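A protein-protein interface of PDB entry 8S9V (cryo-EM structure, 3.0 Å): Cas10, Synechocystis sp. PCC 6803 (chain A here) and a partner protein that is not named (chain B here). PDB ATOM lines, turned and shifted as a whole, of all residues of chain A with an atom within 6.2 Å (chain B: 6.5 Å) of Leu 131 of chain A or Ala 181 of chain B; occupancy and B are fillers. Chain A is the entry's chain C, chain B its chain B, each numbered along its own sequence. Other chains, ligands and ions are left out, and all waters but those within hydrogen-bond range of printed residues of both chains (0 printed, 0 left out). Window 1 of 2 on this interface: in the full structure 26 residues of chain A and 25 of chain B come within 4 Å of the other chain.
CG2 of Thr 127 of chain A touches OD1 of Asn 179 of chain B (3.8 Å).
Lys 128 of chain A touches Cys 180 of chain B (CB to SG, 3.8 Å).
Ile 171 of chain B touches Leu 131 of chain A (CG2 to CD1, 3.6 Å).
Cys 180 of chain B touches Leu 131 of chain A (C to CD1, 3.9 Å).
Leu 131 of chain A touches Ala 181 of chain B (CD1 to CA, 3.8 Å).
Arg 178 of chain A touches Ile 118 of chain B (NH1 to CD1, 3.5 Å).
Gln 120 of chain B touches Arg 178 of chain A (NE2 to NH1, 3.9 Å).
Val 182 of chain B touches Arg 178 of chain A.
The backbone NH (N) of Val 174 of chain B sits at hydrogen-bond distance from the backbone carbonyl oxygen (O) of Asn 179 of chain B, at 2.7 Å.
O of Leu 131 of chain A lies within hydrogen-bond range of NH2 of Arg 178 of chain A (3.2 Å).
The backbone NH (N) of Ala 172 of chain B is in hydrogen-bond range of the backbone carbonyl oxygen (O) of Ala 181 of chain B.
OG1 of Thr 127 of chain A lies within hydrogen-bond range of N of Cys 180 of chain B (3.2 Å).
Of the 15 printed residues of chain A, 4 touch a printed residue of chain B.
Hydrophobic or aromatic side chains of chain A that line the printed part of chain B: Leu 131.
Of the 13 printed residues of chain B, 7 touch a printed residue of chain A.
Along chain B the printed residues that touch a printed residue of chain A span positions 118 to 182.
Among the printed residues, 9 pairs touch across the chains.
Val 126 of chain A touches none of the printed residues of chain B.
Leu 131 of chain A touches just these residues of chain B: Ile 171 (3.6 Å), Cys 180 (3.9 Å) and Ala 181 (3.8 Å).
Ile 139 of chain A touches none of the printed residues of chain B.
Of the printed residues of chain A, Ile 118 of chain B touches Arg 178.
Of the printed residues of chain A, Ile 171 of chain B touches Leu 131.
Ala 181 of chain B touches one residue of chain A.
The nearest printed residue of chain B that does not touch Thr 127 of chain A is Ala 181 of chain B (6.1 Å).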
ATOM      1  N   VAL A 126     -19.868  28.501 -16.079  1.00  0.00           N
ATOM      2  CA  VAL A 126     -20.016  28.483 -14.626  1.00  0.00           C
ATOM      3  C   VAL A 126     -19.672  27.124 -14.035  1.00  0.00           C
ATOM      4  O   VAL A 126     -19.068  27.046 -12.963  1.00  0.00           O
ATOM      5  CB  VAL A 126     -21.439  28.908 -14.233  1.00  0.00           C
ATOM      6  CG1 VAL A 126     -21.619  28.787 -12.748  1.00  0.00           C
ATOM      7  CG2 VAL A 126     -21.706  30.314 -14.680  1.00  0.00           C
ATOM      8  N   THR A 127     -20.100  26.036 -14.678  1.00  0.00           N
ATOM      9  CA  THR A 127     -19.852  24.705 -14.130  1.00  0.00           C
ATOM     10  C   THR A 127     -18.402  24.267 -14.274  1.00  0.00           C
ATOM     11  O   THR A 127     -17.844  23.664 -13.357  1.00  0.00           O
ATOM     12  CB  THR A 127     -20.764  23.695 -14.794  1.00  0.00           C
ATOM     13  OG1 THR A 127     -20.559  23.748 -16.200  1.00  0.00           O
ATOM     14  CG2 THR A 127     -22.181  24.032 -14.519  1.00  0.00           C
ATOM     15  N   LYS A 128     -17.769  24.563 -15.404  1.00  0.00           N
ATOM     16  CA  LYS A 128     -16.340  24.309 -15.552  1.00  0.00           C
ATOM     17  C   LYS A 128     -15.527  24.961 -14.447  1.00  0.00           C
ATOM     18  O   LYS A 128     -14.643  24.336 -13.865  1.00  0.00           O
ATOM     19  CB  LYS A 128     -15.858  24.760 -16.918  1.00  0.00           C
ATOM     20  CG  LYS A 128     -14.385  24.566 -17.122  1.00  0.00           C
ATOM     21  CD  LYS A 128     -13.935  25.192 -18.421  1.00  0.00           C
ATOM     22  CE  LYS A 128     -14.021  26.694 -18.374  1.00  0.00           C
ATOM     23  NZ  LYS A 128     -13.684  27.301 -19.683  1.00  0.00           N
ATOM     24  N   GLN A 129     -15.780  26.231 -14.165  1.00  0.00           N
ATOM     25  CA  GLN A 129     -15.039  26.891 -13.097  1.00  0.00           C
ATOM     26  C   GLN A 129     -15.297  26.249 -11.744  1.00  0.00           C
ATOM     27  O   GLN A 129     -14.423  26.271 -10.877  1.00  0.00           O
ATOM     28  CB  GLN A 129     -15.405  28.367 -13.035  1.00  0.00           C
ATOM     29  CG  GLN A 129     -14.995  29.166 -14.241  1.00  0.00           C
ATOM     30  CD  GLN A 129     -13.562  28.941 -14.632  1.00  0.00           C
ATOM     31  OE1 GLN A 129     -13.251  28.729 -15.802  1.00  0.00           O
ATOM     32  NE2 GLN A 129     -12.670  29.003 -13.658  1.00  0.00           N
ATOM     33  N   ALA A 130     -16.500  25.743 -11.510  1.00  0.00           N
ATOM     34  CA  ALA A 130     -16.757  25.021 -10.270  1.00  0.00           C
ATOM     35  C   ALA A 130     -15.942  23.738 -10.176  1.00  0.00           C
ATOM     36  O   ALA A 130     -15.460  23.387  -9.095  1.00  0.00           O
ATOM     37  CB  ALA A 130     -18.247  24.721 -10.142  1.00  0.00           C
ATOM     38  N   LEU A 131     -15.808  22.999 -11.279  1.00  0.00           N
ATOM     39  CA  LEU A 131     -14.981  21.793 -11.269  1.00  0.00           C
ATOM     40  C   LEU A 131     -13.540  22.091 -10.905  1.00  0.00           C
ATOM     41  O   LEU A 131     -12.882  21.288 -10.240  1.00  0.00           O
ATOM     42  CB  LEU A 131     -15.005  21.107 -12.625  1.00  0.00           C
ATOM     43  CG  LEU A 131     -16.263  20.400 -13.059  1.00  0.00           C
ATOM     44  CD1 LEU A 131     -16.089  19.988 -14.474  1.00  0.00           C
ATOM     45  CD2 LEU A 131     -16.462  19.212 -12.202  1.00  0.00           C
ATOM     46  N   ILE A 132     -13.018  23.219 -11.359  1.00  0.00           N
ATOM     47  CA  ILE A 132     -11.617  23.527 -11.125  1.00  0.00           C
ATOM     48  C   ILE A 132     -11.420  24.187  -9.774  1.00  0.00           C
ATOM     49  O   ILE A 132     -10.629  23.726  -8.949  1.00  0.00           O
ATOM     50  CB  ILE A 132     -11.093  24.423 -12.252  1.00  0.00           C
ATOM     51  CG1 ILE A 132     -11.214  23.714 -13.580  1.00  0.00           C
ATOM     52  CG2 ILE A 132      -9.677  24.801 -11.995  1.00  0.00           C
ATOM     53  CD1 ILE A 132     -11.115  24.639 -14.715  1.00  0.00           C
ATOM     54  N   ASN A 133     -12.137  25.268  -9.528  1.00  0.00           N
ATOM     55  CA  ASN A 133     -11.898  26.122  -8.381  1.00  0.00           C
ATOM     56  C   ASN A 133     -12.645  25.691  -7.134  1.00  0.00           C
ATOM     57  O   ASN A 133     -12.354  26.203  -6.053  1.00  0.00           O
ATOM     58  CB  ASN A 133     -12.249  27.557  -8.744  1.00  0.00           C
ATOM     59  CG  ASN A 133     -11.549  28.014 -10.010  1.00  0.00           C
ATOM     60  OD1 ASN A 133     -12.179  28.518 -10.935  1.00  0.00           O
ATOM     61  ND2 ASN A 133     -10.245  27.812 -10.068  1.00  0.00           N
ATOM     62  N   ALA A 134     -13.624  24.806  -7.258  1.00  0.00           N
ATOM     63  CA  ALA A 134     -14.439  24.367  -6.127  1.00  0.00           C
ATOM     64  C   ALA A 134     -14.739  22.888  -6.277  1.00  0.00           C
ATOM     65  O   ALA A 134     -15.887  22.493  -6.474  1.00  0.00           O
ATOM     66  CB  ALA A 134     -15.726  25.177  -6.027  1.00  0.00           C
ATOM     67  N   PRO A 135     -13.710  22.045  -6.277  1.00  0.00           N
ATOM     68  CA  PRO A 135     -13.939  20.608  -6.425  1.00  0.00           C
ATOM     69  C   PRO A 135     -14.835  20.090  -5.313  1.00  0.00           C
ATOM     70  O   PRO A 135     -14.732  20.518  -4.163  1.00  0.00           O
ATOM     71  CB  PRO A 135     -12.532  20.023  -6.340  1.00  0.00           C
ATOM     72  CG  PRO A 135     -11.785  20.997  -5.553  1.00  0.00           C
ATOM     73  CD  PRO A 135     -12.308  22.327  -5.941  1.00  0.00           C
ATOM     74  N   GLY A 136     -15.721  19.164  -5.659  1.00  0.00           N
ATOM     75  CA  GLY A 136     -16.660  18.626  -4.705  1.00  0.00           C
ATOM     76  C   GLY A 136     -17.891  19.461  -4.446  1.00  0.00           C
ATOM     77  O   GLY A 136     -18.756  19.029  -3.679  1.00  0.00           O
ATOM     78  N   LEU A 137     -17.963  20.669  -4.985  1.00  0.00           N
ATOM     79  CA  LEU A 137     -19.203  21.426  -5.037  1.00  0.00           C
ATOM     80  C   LEU A 137     -20.055  20.895  -6.172  1.00  0.00           C
ATOM     81  O   LEU A 137     -19.575  20.769  -7.298  1.00  0.00           O
ATOM     82  CB  LEU A 137     -18.923  22.906  -5.251  1.00  0.00           C
ATOM     83  CG  LEU A 137     -20.098  23.858  -5.199  1.00  0.00           C
ATOM     84  CD1 LEU A 137     -20.464  24.099  -3.788  1.00  0.00           C
ATOM     85  CD2 LEU A 137     -19.702  25.128  -5.839  1.00  0.00           C
ATOM     86  N   ILE A 139     -22.879  21.613  -8.650  1.00  0.00           N
ATOM     87  CA  ILE A 139     -23.609  22.693  -9.291  1.00  0.00           C
ATOM     88  C   ILE A 139     -23.967  22.281 -10.705  1.00  0.00           C
ATOM     89  O   ILE A 139     -23.199  21.580 -11.370  1.00  0.00           O
ATOM     90  CB  ILE A 139     -22.778  23.986  -9.314  1.00  0.00           C
ATOM     91  CG1 ILE A 139     -23.554  25.093 -10.004  1.00  0.00           C
ATOM     92  CG2 ILE A 139     -21.473  23.765 -10.011  1.00  0.00           C
ATOM     93  CD1 ILE A 139     -22.984  26.447  -9.791  1.00  0.00           C
ATOM     94  N   ALA A 173     -23.942  13.074 -14.554  1.00  0.00           N
ATOM     95  CA  ALA A 173     -22.809  12.546 -13.794  1.00  0.00           C
ATOM     96  C   ALA A 173     -22.650  13.255 -12.450  1.00  0.00           C
ATOM     97  O   ALA A 173     -22.519  14.482 -12.394  1.00  0.00           O
ATOM     98  CB  ALA A 173     -21.532  12.678 -14.619  1.00  0.00           C
ATOM     99  N   ARG A 178     -15.778  11.472  -9.225  1.00  0.00           N
ATOM    100  CA  ARG A 178     -14.385  11.856  -9.368  1.00  0.00           C
ATOM    101  C   ARG A 178     -13.699  11.711  -8.021  1.00  0.00           C
ATOM    102  O   ARG A 178     -14.349  11.646  -6.981  1.00  0.00           O
ATOM    103  CB  ARG A 178     -14.272  13.258  -9.964  1.00  0.00           C
ATOM    104  CG  ARG A 178     -14.660  14.360  -9.054  1.00  0.00           C
ATOM    105  CD  ARG A 178     -14.609  15.689  -9.777  1.00  0.00           C
ATOM    106  NE  ARG A 178     -13.257  16.171 -10.001  1.00  0.00           N
ATOM    107  CZ  ARG A 178     -12.909  17.444  -9.908  1.00  0.00           C
ATOM    108  NH1 ARG A 178     -11.666  17.821 -10.138  1.00  0.00           N
ATOM    109  NH2 ARG A 178     -13.809  18.338  -9.560  1.00  0.00           N
ATOM    110  N   ILE B 118      -6.922  18.636 -15.874  1.00  0.00           N
ATOM    111  CA  ILE B 118      -6.319  19.140 -14.651  1.00  0.00           C
ATOM    112  C   ILE B 118      -5.606  17.985 -13.966  1.00  0.00           C
ATOM    113  O   ILE B 118      -6.164  16.893 -13.845  1.00  0.00           O
ATOM    114  CB  ILE B 118      -7.366  19.790 -13.734  1.00  0.00           C
ATOM    115  CG1 ILE B 118      -8.418  18.791 -13.303  1.00  0.00           C
ATOM    116  CG2 ILE B 118      -8.079  20.895 -14.455  1.00  0.00           C
ATOM    117  CD1 ILE B 118      -9.420  19.385 -12.363  1.00  0.00           C
ATOM    118  N   GLN B 120      -3.942  15.718 -10.952  1.00  0.00           N
ATOM    119  CA  GLN B 120      -4.303  15.305  -9.602  1.00  0.00           C
ATOM    120  C   GLN B 120      -3.229  14.423  -8.992  1.00  0.00           C
ATOM    121  O   GLN B 120      -2.382  13.870  -9.688  1.00  0.00           O
ATOM    122  CB  GLN B 120      -5.625  14.539  -9.591  1.00  0.00           C
ATOM    123  CG  GLN B 120      -6.809  15.374  -9.932  1.00  0.00           C
ATOM    124  CD  GLN B 120      -6.965  16.508  -8.953  1.00  0.00           C
ATOM    125  OE1 GLN B 120      -6.257  16.566  -7.949  1.00  0.00           O
ATOM    126  NE2 GLN B 120      -7.881  17.420  -9.236  1.00  0.00           N
ATOM    127  N   TYR B 170      -9.990  14.755 -17.022  1.00  0.00           N
ATOM    128  CA  TYR B 170     -10.400  15.371 -18.280  1.00  0.00           C
ATOM    129  C   TYR B 170     -11.817  15.905 -18.186  1.00  0.00           C
ATOM    130  O   TYR B 170     -12.749  15.147 -17.929  1.00  0.00           O
ATOM    131  CB  TYR B 170     -10.302  14.388 -19.437  1.00  0.00           C
ATOM    132  CG  TYR B 170      -8.907  13.949 -19.712  1.00  0.00           C
ATOM    133  CD1 TYR B 170      -8.342  12.892 -19.043  1.00  0.00           C
ATOM    134  CD2 TYR B 170      -8.130  14.641 -20.603  1.00  0.00           C
ATOM    135  CE1 TYR B 170      -7.062  12.513 -19.293  1.00  0.00           C
ATOM    136  CE2 TYR B 170      -6.857  14.275 -20.850  1.00  0.00           C
ATOM    137  CZ  TYR B 170      -6.323  13.215 -20.199  1.00  0.00           C
ATOM    138  OH  TYR B 170      -5.032  12.870 -20.479  1.00  0.00           O
ATOM    139  N   ILE B 171     -11.977  17.192 -18.421  1.00  0.00           N
ATOM    140  CA  ILE B 171     -13.235  17.894 -18.225  1.00  0.00           C
ATOM    141  C   ILE B 171     -13.909  18.095 -19.572  1.00  0.00           C
ATOM    142  O   ILE B 171     -13.252  18.479 -20.543  1.00  0.00           O
ATOM    143  CB  ILE B 171     -12.998  19.229 -17.509  1.00  0.00           C
ATOM    144  CG1 ILE B 171     -12.585  18.956 -16.071  1.00  0.00           C
ATOM    145  CG2 ILE B 171     -14.215  20.077 -17.569  1.00  0.00           C
ATOM    146  CD1 ILE B 171     -12.195  20.142 -15.331  1.00  0.00           C
ATOM    147  N   ALA B 172     -15.201  17.797 -19.654  1.00  0.00           N
ATOM    148  CA  ALA B 172     -15.925  18.005 -20.897  1.00  0.00           C
ATOM    149  C   ALA B 172     -17.388  18.276 -20.598  1.00  0.00           C
ATOM    150  O   ALA B 172     -17.866  18.029 -19.492  1.00  0.00           O
ATOM    151  CB  ALA B 172     -15.799  16.803 -21.823  1.00  0.00           C
ATOM    152  N   GLU B 173     -18.092  18.811 -21.594  1.00  0.00           N
ATOM    153  CA  GLU B 173     -19.543  18.967 -21.512  1.00  0.00           C
ATOM    154  C   GLU B 173     -20.232  17.613 -21.527  1.00  0.00           C
ATOM    155  O   GLU B 173     -20.032  16.813 -22.443  1.00  0.00           O
ATOM    156  CB  GLU B 173     -20.059  19.835 -22.650  1.00  0.00           C
ATOM    157  CG  GLU B 173     -19.574  21.253 -22.573  1.00  0.00           C
ATOM    158  CD  GLU B 173     -19.934  22.051 -23.793  1.00  0.00           C
ATOM    159  OE1 GLU B 173     -21.103  21.978 -24.227  1.00  0.00           O
ATOM    160  OE2 GLU B 173     -19.047  22.748 -24.325  1.00  0.00           O
ATOM    161  N   VAL B 174     -21.086  17.378 -20.539  1.00  0.00           N
ATOM    162  CA  VAL B 174     -21.903  16.178 -20.487  1.00  0.00           C
ATOM    163  C   VAL B 174     -23.316  16.405 -21.016  1.00  0.00           C
ATOM    164  O   VAL B 174     -23.756  15.713 -21.931  1.00  0.00           O
ATOM    165  CB  VAL B 174     -21.932  15.662 -19.033  1.00  0.00           C
ATOM    166  CG1 VAL B 174     -22.821  14.458 -18.925  1.00  0.00           C
ATOM    167  CG2 VAL B 174     -20.534  15.353 -18.563  1.00  0.00           C
ATOM    168  N   ASN B 179     -23.674  21.448 -19.136  1.00  0.00           N
ATOM    169  CA  ASN B 179     -23.040  21.087 -17.877  1.00  0.00           C
ATOM    170  C   ASN B 179     -21.727  20.355 -18.118  1.00  0.00           C
ATOM    171  O   ASN B 179     -21.708  19.312 -18.768  1.00  0.00           O
ATOM    172  CB  ASN B 179     -23.974  20.205 -17.066  1.00  0.00           C
ATOM    173  CG  ASN B 179     -25.167  20.945 -16.553  1.00  0.00           C
ATOM    174  OD1 ASN B 179     -25.041  21.838 -15.729  1.00  0.00           O
ATOM    175  ND2 ASN B 179     -26.343  20.571 -17.028  1.00  0.00           N
ATOM    176  N   CYS B 180     -20.631  20.888 -17.588  1.00  0.00           N
ATOM    177  CA  CYS B 180     -19.342  20.209 -17.662  1.00  0.00           C
ATOM    178  C   CYS B 180     -19.217  19.129 -16.591  1.00  0.00           C
ATOM    179  O   CYS B 180     -19.784  19.239 -15.502  1.00  0.00           O
ATOM    180  CB  CYS B 180     -18.204  21.207 -17.520  1.00  0.00           C
ATOM    181  SG  CYS B 180     -18.055  22.345 -18.878  1.00  0.00           S
ATOM    182  N   ALA B 181     -18.441  18.089 -16.902  1.00  0.00           N
ATOM    183  CA  ALA B 181     -18.019  17.099 -15.919  1.00  0.00           C
ATOM    184  C   ALA B 181     -16.673  16.526 -16.336  1.00  0.00           C
ATOM    185  O   ALA B 181     -16.202  16.766 -17.446  1.00  0.00           O
ATOM    186  CB  ALA B 181     -19.056  15.990 -15.775  1.00  0.00           C
ATOM    187  N   VAL B 182     -16.050  15.766 -15.434  1.00  0.00           N
ATOM    188  CA  VAL B 182     -14.862  14.981 -15.768  1.00  0.00           C
ATOM    189  C   VAL B 182     -15.263  13.681 -16.448  1.00  0.00           C
ATOM    190  O   VAL B 182     -15.906  12.823 -15.842  1.00  0.00           O
ATOM    191  CB  VAL B 182     -14.015  14.698 -14.526  1.00  0.00           C
ATOM    192  CG1 VAL B 182     -13.502  15.968 -13.948  1.00  0.00           C
ATOM    193  CG2 VAL B 182     -14.832  13.996 -13.525  1.00  0.00           C
ATOM    194  N   ILE B 183     -14.837  13.515 -17.693  1.00  0.00           N
ATOM    195  CA  ILE B 183     -15.174  12.341 -18.481  1.00  0.00           C
ATOM    196  C   ILE B 183     -14.232  11.153 -18.324  1.00  0.00           C
ATOM    197  O   ILE B 183     -14.589  10.042 -18.738  1.00  0.00           O
ATOM    198  CB  ILE B 183     -15.190  12.728 -19.961  1.00  0.00           C
ATOM    199  CG1 ILE B 183     -13.839  13.325 -20.326  1.00  0.00           C
ATOM    200  CG2 ILE B 183     -16.268  13.721 -20.221  1.00  0.00           C
ATOM    201  CD1 ILE B 183     -13.526  13.251 -21.779  1.00  0.00           C
ATOM    202  N   ASP B 184     -13.035  11.350 -17.778  1.00  0.00           N
ATOM    203  CA  ASP B 184     -12.172  10.233 -17.425  1.00  0.00           C
ATOM    204  C   ASP B 184     -11.137  10.743 -16.441  1.00  0.00           C
ATOM    205  O   ASP B 184     -10.938  11.948 -16.316  1.00  0.00           O
ATOM    206  CB  ASP B 184     -11.525   9.630 -18.669  1.00  0.00           C
ATOM    207  CG  ASP B 184     -10.988   8.242 -18.432  1.00  0.00           C
ATOM    208  OD1 ASP B 184     -11.801   7.340 -18.153  1.00  0.00           O
ATOM    209  OD2 ASP B 184      -9.761   8.042 -18.550  1.00  0.00           O
